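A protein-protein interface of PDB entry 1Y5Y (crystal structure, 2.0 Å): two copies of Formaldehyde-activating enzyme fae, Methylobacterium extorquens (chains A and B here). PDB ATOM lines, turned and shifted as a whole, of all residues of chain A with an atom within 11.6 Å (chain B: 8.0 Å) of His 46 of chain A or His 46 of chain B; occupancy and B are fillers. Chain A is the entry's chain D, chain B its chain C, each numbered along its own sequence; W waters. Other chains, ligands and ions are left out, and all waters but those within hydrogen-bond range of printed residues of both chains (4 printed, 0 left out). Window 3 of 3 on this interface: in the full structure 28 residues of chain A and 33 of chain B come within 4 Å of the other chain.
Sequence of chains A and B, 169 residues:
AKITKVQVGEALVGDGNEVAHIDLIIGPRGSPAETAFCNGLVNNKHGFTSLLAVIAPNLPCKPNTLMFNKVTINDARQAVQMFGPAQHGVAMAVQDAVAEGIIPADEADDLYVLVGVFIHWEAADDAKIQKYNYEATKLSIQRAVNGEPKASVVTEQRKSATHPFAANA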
ATOM      1  N   GLY A  40       3.649  -6.113  20.211  1.00  0.00           N
ATOM      2  CA  GLY A  40       3.310  -7.470  20.561  1.00  0.00           C
ATOM      3  C   GLY A  40       3.124  -7.692  22.063  1.00  0.00           C
ATOM      4  O   GLY A  40       2.297  -8.489  22.484  1.00  0.00           O
ATOM      5  N   VAL A  42       1.992  -5.444  24.105  1.00  0.00           N
ATOM      6  CA  VAL A  42       0.766  -4.721  24.441  1.00  0.00           C
ATOM      7  C   VAL A  42      -0.562  -5.358  23.976  1.00  0.00           C
ATOM      8  O   VAL A  42      -1.570  -5.343  24.691  1.00  0.00           O
ATOM      9  CB  VAL A  42       0.842  -3.293  23.843  1.00  0.00           C
ATOM     10  CG1 VAL A  42      -0.517  -2.562  23.987  1.00  0.00           C
ATOM     11  CG2 VAL A  42       1.992  -2.491  24.553  1.00  0.00           C
ATOM     12  N   ASN A  43      -0.537  -5.952  22.794  1.00  0.00           N
ATOM     13  CA  ASN A  43      -1.741  -6.493  22.145  1.00  0.00           C
ATOM     14  C   ASN A  43      -1.981  -7.989  22.386  1.00  0.00           C
ATOM     15  O   ASN A  43      -1.363  -8.824  21.734  1.00  0.00           O
ATOM     16  CB  ASN A  43      -1.604  -6.148  20.634  1.00  0.00           C
ATOM     17  CG  ASN A  43      -2.786  -6.653  19.760  1.00  0.00           C
ATOM     18  OD1 ASN A  43      -2.719  -6.631  18.528  1.00  0.00           O
ATOM     19  ND2 ASN A  43      -3.832  -7.089  20.380  1.00  0.00           N
ATOM     20  N   ASN A  44      -2.818  -8.330  23.357  1.00  0.00           N
ATOM     21  CA  ASN A  44      -3.128  -9.741  23.617  1.00  0.00           C
ATOM     22  C   ASN A  44      -4.640 -10.024  23.426  1.00  0.00           C
ATOM     23  O   ASN A  44      -5.441  -9.094  23.400  1.00  0.00           O
ATOM     24  CB  ASN A  44      -2.721 -10.176  25.015  1.00  0.00           C
ATOM     25  CG  ASN A  44      -1.195 -10.344  25.186  1.00  0.00           C
ATOM     26  OD1 ASN A  44      -0.390 -10.275  24.223  1.00  0.00           O
ATOM     27  ND2 ASN A  44      -0.796 -10.566  26.422  1.00  0.00           N
ATOM     28  N   LYS A  45      -5.015 -11.302  23.303  1.00  0.00           N
ATOM     29  CA  LYS A  45      -6.429 -11.684  23.058  1.00  0.00           C
ATOM     30  C   LYS A  45      -6.719 -12.980  23.729  1.00  0.00           C
ATOM     31  O   LYS A  45      -5.790 -13.682  24.200  1.00  0.00           O
ATOM     32  CB  LYS A  45      -6.713 -11.955  21.549  1.00  0.00           C
ATOM     33  CG  LYS A  45      -6.015 -11.077  20.536  1.00  0.00           C
ATOM     34  CD  LYS A  45      -4.645 -11.687  20.219  1.00  0.00           C
ATOM     35  CE  LYS A  45      -3.762 -10.724  19.433  1.00  0.00           C
ATOM     36  NZ  LYS A  45      -2.393 -11.309  19.286  1.00  0.00           N
ATOM     37  N   HIS A  46      -7.993 -13.352  23.733  1.00  0.00           N
ATOM     38  CA  HIS A  46      -8.413 -14.613  24.333  1.00  0.00           C
ATOM     39  C   HIS A  46      -7.602 -15.742  23.702  1.00  0.00           C
ATOM     40  O   HIS A  46      -7.563 -15.858  22.477  1.00  0.00           O
ATOM     41  CB  HIS A  46      -9.901 -14.859  24.058  1.00  0.00           C
ATOM     42  CG  HIS A  46     -10.828 -14.035  24.900  1.00  0.00           C
ATOM     43  ND1 HIS A  46     -12.141 -13.798  24.549  1.00  0.00           N
ATOM     44  CD2 HIS A  46     -10.657 -13.460  26.112  1.00  0.00           C
ATOM     45  CE1 HIS A  46     -12.739 -13.117  25.512  1.00  0.00           C
ATOM     46  NE2 HIS A  46     -11.860 -12.901  26.472  1.00  0.00           N
ATOM     47  N   GLY A  47      -6.949 -16.553  24.533  1.00  0.00           N
ATOM     48  CA  GLY A  47      -6.178 -17.693  24.026  1.00  0.00           C
ATOM     49  C   GLY A  47      -4.820 -17.426  23.397  1.00  0.00           C
ATOM     50  O   GLY A  47      -4.077 -18.394  23.102  1.00  0.00           O
ATOM     51  N   PHE A  48      -4.486 -16.158  23.214  1.00  0.00           N
ATOM     52  CA  PHE A  48      -3.221 -15.750  22.546  1.00  0.00           C
ATOM     53  C   PHE A  48      -2.488 -14.705  23.342  1.00  0.00           C
ATOM     54  O   PHE A  48      -2.819 -13.516  23.329  1.00  0.00           O
ATOM     55  CB  PHE A  48      -3.481 -15.235  21.113  1.00  0.00           C
ATOM     56  CG  PHE A  48      -3.790 -16.347  20.161  1.00  0.00           C
ATOM     57  CD1 PHE A  48      -5.085 -16.856  20.071  1.00  0.00           C
ATOM     58  CD2 PHE A  48      -2.757 -16.997  19.478  1.00  0.00           C
ATOM     59  CE1 PHE A  48      -5.361 -18.006  19.327  1.00  0.00           C
ATOM     60  CE2 PHE A  48      -3.021 -18.164  18.717  1.00  0.00           C
ATOM     61  CZ  PHE A  48      -4.337 -18.671  18.646  1.00  0.00           C
ATOM     62  N   THR A  49      -1.474 -15.175  24.028  1.00  0.00           N
ATOM     63  CA  THR A  49      -0.717 -14.315  24.905  1.00  0.00           C
ATOM     64  C   THR A  49       0.685 -14.027  24.381  1.00  0.00           C
ATOM     65  O   THR A  49       1.132 -14.555  23.339  1.00  0.00           O
ATOM     66  CB  THR A  49      -0.626 -14.996  26.308  1.00  0.00           C
ATOM     67  OG1 THR A  49      -0.219 -14.033  27.300  1.00  0.00           O
ATOM     68  CG2 THR A  49       0.413 -16.144  26.270  1.00  0.00           C
ATOM     69  N   SER A  50       1.374 -13.163  25.107  1.00  0.00           N
ATOM     70  CA  SER A  50       2.736 -12.870  24.796  1.00  0.00           C
ATOM     71  C   SER A  50       3.377 -12.540  26.136  1.00  0.00           C
ATOM     72  O   SER A  50       2.749 -11.939  27.027  1.00  0.00           O
ATOM     73  CB  SER A  50       2.853 -11.697  23.836  1.00  0.00           C
ATOM     74  OG  SER A  50       2.559 -10.461  24.439  1.00  0.00           O
ATOM     75  N   PHE A  68       5.447 -15.779  22.148  1.00  0.00           N
ATOM     76  CA  PHE A  68       3.990 -15.832  21.980  1.00  0.00           C
ATOM     77  C   PHE A  68       3.602 -17.190  21.438  1.00  0.00           C
ATOM     78  O   PHE A  68       4.366 -17.798  20.680  1.00  0.00           O
ATOM     79  CB  PHE A  68       3.498 -14.708  21.045  1.00  0.00           C
ATOM     80  CG  PHE A  68       4.392 -14.476  19.874  1.00  0.00           C
ATOM     81  CD1 PHE A  68       4.192 -15.153  18.679  1.00  0.00           C
ATOM     82  CD2 PHE A  68       5.513 -13.644  20.006  1.00  0.00           C
ATOM     83  CE1 PHE A  68       5.105 -15.013  17.629  1.00  0.00           C
ATOM     84  CE2 PHE A  68       6.436 -13.492  18.960  1.00  0.00           C
ATOM     85  CZ  PHE A  68       6.240 -14.173  17.779  1.00  0.00           C
ATOM     86  N   ASN A  69       2.430 -17.674  21.830  1.00  0.00           N
ATOM     87  CA  ASN A  69       1.961 -18.979  21.390  1.00  0.00           C
ATOM     88  C   ASN A  69       1.274 -18.920  20.024  1.00  0.00           C
ATOM     89  O   ASN A  69       0.619 -17.932  19.694  1.00  0.00           O
ATOM     90  CB  ASN A  69       0.976 -19.580  22.404  1.00  0.00           C
ATOM     91  CG  ASN A  69      -0.245 -18.659  22.660  1.00  0.00           C
ATOM     92  OD1 ASN A  69      -0.090 -17.514  23.066  1.00  0.00           O
ATOM     93  ND2 ASN A  69      -1.446 -19.163  22.408  1.00  0.00           N
ATOM     94  N   LYS A  70       1.442 -20.009  19.258  1.00  0.00           N
ATOM     95  CA  LYS A  70       0.823 -20.192  17.942  1.00  0.00           C
ATOM     96  C   LYS A  70      -0.381 -21.109  18.077  1.00  0.00           C
ATOM     97  O   LYS A  70      -1.277 -21.065  17.259  1.00  0.00           O
ATOM     98  CB  LYS A  70       1.810 -20.831  16.964  1.00  0.00           C
ATOM     99  CG  LYS A  70       2.882 -19.860  16.504  1.00  0.00           C
ATOM    100  CD  LYS A  70       2.207 -18.716  15.783  1.00  0.00           C
ATOM    101  CE  LYS A  70       3.189 -17.807  15.035  1.00  0.00           C
ATOM    102  NZ  LYS A  70       2.383 -16.841  14.203  1.00  0.00           N
ATOM    103  N   VAL A  71      -0.407 -21.953  19.100  1.00  0.00           N
ATOM    104  CA  VAL A  71      -1.561 -22.846  19.278  1.00  0.00           C
ATOM    105  C   VAL A  71      -2.408 -22.238  20.398  1.00  0.00           C
ATOM    106  O   VAL A  71      -1.876 -21.833  21.436  1.00  0.00           O
ATOM    107  CB  VAL A  71      -1.127 -24.263  19.683  1.00  0.00           C
ATOM    108  CG1 VAL A  71      -2.362 -25.118  20.037  1.00  0.00           C
ATOM    109  CG2 VAL A  71      -0.316 -24.902  18.535  1.00  0.00           C
ATOM    110  N   THR A  72      -3.712 -22.151  20.175  1.00  0.00           N
ATOM    111  CA  THR A  72      -4.627 -21.580  21.158  1.00  0.00           C
ATOM    112  C   THR A  72      -4.485 -22.194  22.549  1.00  0.00           C
ATOM    113  O   THR A  72      -4.488 -23.410  22.720  1.00  0.00           O
ATOM    114  CB  THR A  72      -6.108 -21.803  20.765  1.00  0.00           C
ATOM    115  OG1 THR A  72      -6.306 -21.455  19.405  1.00  0.00           O
ATOM    116  CG2 THR A  72      -7.015 -20.909  21.613  1.00  0.00           C
ATOM    117  N   ILE A  73      -4.430 -21.344  23.557  1.00  0.00           N
ATOM    118  CA  ILE A  73      -4.349 -21.834  24.922  1.00  0.00           C
ATOM    119  C   ILE A  73      -5.802 -21.906  25.404  1.00  0.00           C
ATOM    120  O   ILE A  73      -6.460 -20.886  25.605  1.00  0.00           O
ATOM    121  CB  ILE A  73      -3.476 -20.870  25.780  1.00  0.00           C
ATOM    122  CG1 ILE A  73      -2.017 -21.083  25.385  1.00  0.00           C
ATOM    123  CG2 ILE A  73      -3.631 -21.163  27.317  1.00  0.00           C
ATOM    124  CD1 ILE A  73      -1.076 -19.914  25.824  1.00  0.00           C
ATOM    125  N   ASN A  74      -6.308 -23.125  25.543  1.00  0.00           N
ATOM    126  CA  ASN A  74      -7.685 -23.317  25.970  1.00  0.00           C
ATOM    127  C   ASN A  74      -7.846 -23.680  27.428  1.00  0.00           C
ATOM    128  O   ASN A  74      -8.949 -23.576  27.967  1.00  0.00           O
ATOM    129  CB  ASN A  74      -8.350 -24.410  25.135  1.00  0.00           C
ATOM    130  CG  ASN A  74      -8.561 -23.989  23.696  1.00  0.00           C
ATOM    131  OD1 ASN A  74      -9.288 -23.028  23.420  1.00  0.00           O
ATOM    132  ND2 ASN A  74      -7.920 -24.698  22.770  1.00  0.00           N
ATOM    133  N   ASP A  75      -6.790 -24.142  28.081  1.00  0.00           N
ATOM    134  CA  ASP A  75      -6.966 -24.472  29.473  1.00  0.00           C
ATOM    135  C   ASP A  75      -5.702 -24.285  30.256  1.00  0.00           C
ATOM    136  O   ASP A  75      -4.658 -23.964  29.677  1.00  0.00           O
ATOM    137  CB  ASP A  75      -7.544 -25.891  29.633  1.00  0.00           C
ATOM    138  CG  ASP A  75      -6.575 -27.007  29.230  1.00  0.00           C
ATOM    139  OD1 ASP A  75      -5.379 -26.781  28.928  1.00  0.00           O
ATOM    140  OD2 ASP A  75      -7.036 -28.163  29.226  1.00  0.00           O
ATOM    141  N   GLN A  78      -2.410 -26.050  29.263  1.00  0.00           N
ATOM    142  CA  GLN A  78      -1.634 -25.456  28.181  1.00  0.00           C
ATOM    143  C   GLN A  78      -0.962 -24.154  28.614  1.00  0.00           C
ATOM    144  O   GLN A  78       0.135 -23.865  28.161  1.00  0.00           O
ATOM    145  CB  GLN A  78      -2.537 -25.202  26.977  1.00  0.00           C
ATOM    146  CG  GLN A  78      -3.004 -26.485  26.281  1.00  0.00           C
ATOM    147  CD  GLN A  78      -4.012 -26.171  25.202  1.00  0.00           C
ATOM    148  OE1 GLN A  78      -5.054 -25.569  25.464  1.00  0.00           O
ATOM    149  NE2 GLN A  78      -3.702 -26.562  23.980  1.00  0.00           N
ATOM    150  N   ALA A  79      -1.622 -23.365  29.469  1.00  0.00           N
ATOM    151  CA  ALA A  79      -1.000 -22.117  29.944  1.00  0.00           C
ATOM    152  C   ALA A  79       0.256 -22.470  30.751  1.00  0.00           C
ATOM    153  O   ALA A  79       1.309 -21.832  30.613  1.00  0.00           O
ATOM    154  CB  ALA A  79      -1.974 -21.301  30.812  1.00  0.00           C
ATOM    155  N   PHE A  83       4.057 -21.159  29.994  1.00  0.00           N
ATOM    156  CA  PHE A  83       4.780 -20.386  30.989  1.00  0.00           C
ATOM    157  C   PHE A  83       5.863 -21.096  31.760  1.00  0.00           C
ATOM    158  O   PHE A  83       6.765 -20.439  32.264  1.00  0.00           O
ATOM    159  CB  PHE A  83       3.786 -19.753  31.975  1.00  0.00           C
ATOM    160  CG  PHE A  83       2.918 -18.697  31.345  1.00  0.00           C
ATOM    161  CD1 PHE A  83       1.711 -19.032  30.753  1.00  0.00           C
ATOM    162  CD2 PHE A  83       3.332 -17.369  31.317  1.00  0.00           C
ATOM    163  CE1 PHE A  83       0.916 -18.064  30.136  1.00  0.00           C
ATOM    164  CE2 PHE A  83       2.549 -16.384  30.705  1.00  0.00           C
ATOM    165  CZ  PHE A  83       1.335 -16.735  30.111  1.00  0.00           C
ATOM    166  N   ASN B  44      -8.720  -2.291  21.456  1.00  0.00           N
ATOM    167  CA  ASN B  44      -9.159  -3.127  22.571  1.00  0.00           C
ATOM    168  C   ASN B  44     -10.027  -4.263  22.023  1.00  0.00           C
ATOM    169  O   ASN B  44     -10.529  -4.180  20.894  1.00  0.00           O
ATOM    170  CB  ASN B  44      -9.966  -2.325  23.620  1.00  0.00           C
ATOM    171  CG  ASN B  44      -9.065  -1.425  24.518  1.00  0.00           C
ATOM    172  OD1 ASN B  44      -7.830  -1.392  24.364  1.00  0.00           O
ATOM    173  ND2 ASN B  44      -9.682  -0.696  25.430  1.00  0.00           N
ATOM    174  N   LYS B  45     -10.246  -5.281  22.850  1.00  0.00           N
ATOM    175  CA  LYS B  45     -11.076  -6.436  22.495  1.00  0.00           C
ATOM    176  C   LYS B  45     -11.694  -7.142  23.699  1.00  0.00           C
ATOM    177  O   LYS B  45     -11.304  -6.894  24.848  1.00  0.00           O
ATOM    178  CB  LYS B  45     -10.285  -7.464  21.658  1.00  0.00           C
ATOM    179  CG  LYS B  45      -8.816  -7.665  22.007  1.00  0.00           C
ATOM    180  CD  LYS B  45      -7.998  -6.467  21.562  1.00  0.00           C
ATOM    181  CE  LYS B  45      -6.496  -6.710  21.562  1.00  0.00           C
ATOM    182  NZ  LYS B  45      -5.830  -6.230  22.764  1.00  0.00           N
ATOM    183  N   HIS B  46     -12.653  -8.033  23.430  1.00  0.00           N
ATOM    184  CA  HIS B  46     -13.342  -8.770  24.493  1.00  0.00           C
ATOM    185  C   HIS B  46     -12.365  -9.277  25.538  1.00  0.00           C
ATOM    186  O   HIS B  46     -11.497 -10.112  25.238  1.00  0.00           O
ATOM    187  CB  HIS B  46     -14.119  -9.973  23.918  1.00  0.00           C
ATOM    188  CG  HIS B  46     -15.389  -9.602  23.212  1.00  0.00           C
ATOM    189  ND1 HIS B  46     -16.063 -10.474  22.383  1.00  0.00           N
ATOM    190  CD2 HIS B  46     -16.128  -8.467  23.243  1.00  0.00           C
ATOM    191  CE1 HIS B  46     -17.163  -9.893  21.936  1.00  0.00           C
ATOM    192  NE2 HIS B  46     -17.226  -8.674  22.441  1.00  0.00           N
ATOM    193  N   GLY B  47     -12.511  -8.787  26.769  1.00  0.00           N
ATOM    194  CA  GLY B  47     -11.622  -9.238  27.821  1.00  0.00           C
ATOM    195  C   GLY B  47     -10.275  -8.548  27.926  1.00  0.00           C
ATOM    196  O   GLY B  47      -9.592  -8.739  28.927  1.00  0.00           O
ATOM    197  N   PHE B  48      -9.899  -7.722  26.944  1.00  0.00           N
ATOM    198  CA  PHE B  48      -8.565  -7.081  26.965  1.00  0.00           C
ATOM    199  C   PHE B  48      -8.684  -5.609  26.723  1.00  0.00           C
ATOM    200  O   PHE B  48      -8.931  -5.139  25.614  1.00  0.00           O
ATOM    201  CB  PHE B  48      -7.628  -7.751  25.935  1.00  0.00           C
ATOM    202  CG  PHE B  48      -7.199  -9.130  26.355  1.00  0.00           C
ATOM    203  CD1 PHE B  48      -7.994 -10.240  26.093  1.00  0.00           C
ATOM    204  CD2 PHE B  48      -6.033  -9.310  27.091  1.00  0.00           C
ATOM    205  CE1 PHE B  48      -7.621 -11.521  26.564  1.00  0.00           C
ATOM    206  CE2 PHE B  48      -5.660 -10.575  27.572  1.00  0.00           C
ATOM    207  CZ  PHE B  48      -6.455 -11.681  27.306  1.00  0.00           C
ATOM    208  N   THR B  49      -8.502  -4.869  27.804  1.00  0.00           N
ATOM    209  CA  THR B  49      -8.666  -3.420  27.771  1.00  0.00           C
ATOM    210  C   THR B  49      -7.345  -2.666  27.949  1.00  0.00           C
ATOM    211  O   THR B  49      -6.288  -3.253  28.266  1.00  0.00           O
ATOM    212  CB  THR B  49      -9.624  -3.038  28.954  1.00  0.00           C
ATOM    213  OG1 THR B  49     -10.178  -1.741  28.746  1.00  0.00           O
ATOM    214  CG2 THR B  49      -8.833  -3.024  30.311  1.00  0.00           C
ATOM    215  N   ASN B  69      -4.365  -5.074  30.581  1.00  0.00           N
ATOM    216  CA  ASN B  69      -4.300  -6.377  31.245  1.00  0.00           C
ATOM    217  C   ASN B  69      -3.773  -7.484  30.359  1.00  0.00           C
ATOM    218  O   ASN B  69      -3.998  -7.489  29.145  1.00  0.00           O
ATOM    219  CB  ASN B  69      -5.652  -6.811  31.787  1.00  0.00           C
ATOM    220  CG  ASN B  69      -6.722  -6.867  30.700  1.00  0.00           C
ATOM    221  OD1 ASN B  69      -6.952  -5.889  30.028  1.00  0.00           O
ATOM    222  ND2 ASN B  69      -7.356  -8.026  30.531  1.00  0.00           N
ATOM    223  N   VAL B  71      -4.241 -10.754  31.692  1.00  0.00           N
ATOM    224  CA  VAL B  71      -5.109 -11.864  32.055  1.00  0.00           C
ATOM    225  C   VAL B  71      -6.524 -11.416  31.659  1.00  0.00           C
ATOM    226  O   VAL B  71      -6.960 -10.327  32.033  1.00  0.00           O
ATOM    227  CB  VAL B  71      -5.081 -12.154  33.565  1.00  0.00           C
ATOM    228  CG1 VAL B  71      -6.238 -13.107  33.931  1.00  0.00           C
ATOM    229  CG2 VAL B  71      -3.752 -12.772  33.930  1.00  0.00           C
ATOM    230  N   THR B  72      -7.231 -12.274  30.930  1.00  0.00           N
ATOM    231  CA  THR B  72      -8.583 -11.991  30.476  1.00  0.00           C
ATOM    232  C   THR B  72      -9.489 -11.485  31.606  1.00  0.00           C
ATOM    233  O   THR B  72      -9.493 -12.049  32.698  1.00  0.00           O
ATOM    234  CB  THR B  72      -9.242 -13.262  29.908  1.00  0.00           C
ATOM    235  OG1 THR B  72      -8.418 -13.816  28.874  1.00  0.00           O
ATOM    236  CG2 THR B  72     -10.598 -12.940  29.348  1.00  0.00           C
ATOM    237  N   ILE B  73     -10.252 -10.423  31.343  1.00  0.00           N
ATOM    238  CA  ILE B  73     -11.184  -9.917  32.347  1.00  0.00           C
ATOM    239  C   ILE B  73     -12.540 -10.459  31.892  1.00  0.00           C
ATOM    240  O   ILE B  73     -13.056 -10.043  30.865  1.00  0.00           O
ATOM    241  CB  ILE B  73     -11.151  -8.400  32.354  1.00  0.00           C
ATOM    242  CG1 ILE B  73      -9.815  -7.956  32.960  1.00  0.00           C
ATOM    243  CG2 ILE B  73     -12.355  -7.823  33.194  1.00  0.00           C
ATOM    244  CD1 ILE B  73      -9.543  -6.468  32.806  1.00  0.00           C
ATOM    245  N   ASN B  74     -13.084 -11.431  32.619  1.00  0.00           N
ATOM    246  CA  ASN B  74     -14.367 -12.054  32.213  1.00  0.00           C
ATOM    247  C   ASN B  74     -15.603 -11.578  32.962  1.00  0.00           C
ATOM    248  O   ASN B  74     -16.715 -11.850  32.528  1.00  0.00           O
ATOM    249  CB  ASN B  74     -14.316 -13.586  32.365  1.00  0.00           C
ATOM    250  CG  ASN B  74     -13.292 -14.227  31.461  1.00  0.00           C
ATOM    251  OD1 ASN B  74     -13.031 -13.729  30.362  1.00  0.00           O
ATOM    252  ND2 ASN B  74     -12.708 -15.344  31.910  1.00  0.00           N
HETATM  253  O   HOH W   1      -7.197 -15.897  27.352  1.00  0.00           O
HETATM  254  O   HOH W   2      -4.149  -6.100  24.958  1.00  0.00           O
HETATM  255  O   HOH W   3      -9.977 -11.331  23.045  1.00  0.00           O
HETATM  256  O   HOH W   4     -13.840 -11.911  28.083  1.00  0.00           O
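Of the printed residues of chain B, His 46 of chain A touches His 46, Gly 47, Phe 48 and Thr 72.
Of the printed residues of chain A, His 46 of chain B touches His 46 (3.1 Å).
Printed residues of chain A within 4 Å of Lys 45 of chain B: Asn 43 and Asn 44.
Of the printed residues of chain B, Lys 45 of chain A touches Phe 48 (3.3 Å).
Of the printed residues of chain A, Thr 72 of chain B touches His 46 (3.1 Å).
Of the printed residues of chain A, Phe 48 of chain B touches Asn 44, Lys 45 and His 46.
Of the printed residues of chain B, Asn 44 of chain A touches Lys 45 (3.0 Å) and Phe 48 (3.4 Å).
Ile 73 of chain B touches none of the printed residues of chain A.
The nearest printed residue of chain B that does not touch His 46 of chain A is Asn 74 of chain B (4.1 Å).
The nearest printed residue of chain A that does not touch Lys 45 of chain B is Lys 45 of chain A (4.5 Å).
Asn 44 of chain A touches Lys 45 of chain B, but with the chains exchanged Lys 45 of chain A does not touch Asn 44 of chain B (8.0 Å).
Asn 44 of chain A touches Phe 48 of chain B, but with the chains exchanged Phe 48 of chain A does not touch Asn 44 of chain B (11.8 Å).
Lys 45 of chain A touches Phe 48 of chain B, but with the chains exchanged Phe 48 of chain A does not touch Lys 45 of chain B (7.9 Å).
His 46 of chain A touches Phe 48 of chain B, but with the chains exchanged Phe 48 of chain A does not touch His 46 of chain B (9.5 Å).
The backbone carbonyl oxygen of Gly 47 of chain B lies within hydrogen-bond range of the side-chain amide nitrogen of Asn 69 of chain B (2.8 Å).
The side-chain amide oxygen (OD1) of Asn 44 of chain A is in hydrogen-bond range of the side-chain hydroxyl (OG) of Ser 50 of chain A, 3.0 Å away.
The backbone NH (N) of Ile 73 of chain B is in hydrogen-bond range of the backbone carbonyl oxygen (O) of Gly 47 of chain B (3.0 Å).
Water W2 lies within hydrogen-bond range of O of Val 42 of chain A, NZ of Lys 45 of chain B and N of Asn 44 of chain A.
Water W4 lies within hydrogen-bond range of NE2 of His 46 of chain A (2.7 Å), OD1 of Asn 74 of chain B (3.0 Å) and O of Ile 73 of chain B (3.4 Å).
Water W1 lies within hydrogen-bond range of OG1 of Thr 72 of chain B (2.9 Å) and N of Gly 47 of chain A (2.9 Å).
Water W3 bridges the backbone NH (N) of His 46 of chain A (2.9 Å) and the backbone carbonyl oxygen (O) of His 46 of chain B (2.9 Å).
CG of Phe 48 of chain B touches O of Asn 44 of chain A, at 3.4 Å.
Phe 48 of chain B touches Lys 45 of chain A (CE1 to C, 3.3 Å).
Gly 47 of chain B touches His 46 of chain A (CA to NE2, 3.9 Å).
His 46 of chain A touches Phe 48 of chain B.
NE2 of His 46 of chain A touches CG2 of Thr 72 of chain B, 3.1 Å away.
Hydrophobic or aromatic side chains of chain B within 4 Å of the printed part of chain A: His 46 and Phe 48.
Of the 21 printed residues of chain A, 4 touch a printed residue of chain B.
O of Asn 44 of chain A lies within hydrogen-bond range of NZ of Lys 45 of chain B (3.0 Å).
The backbone carbonyl oxygen (O) of His 46 of chain B is in hydrogen-bond range of a ring nitrogen (NE2) of His 46 of chain A (3.1 Å).
The side-chain amino group of Lys 45 of chain B sits close to the side-chain amide nitrogen of Asn 43 of chain A, 3.2 Å away.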
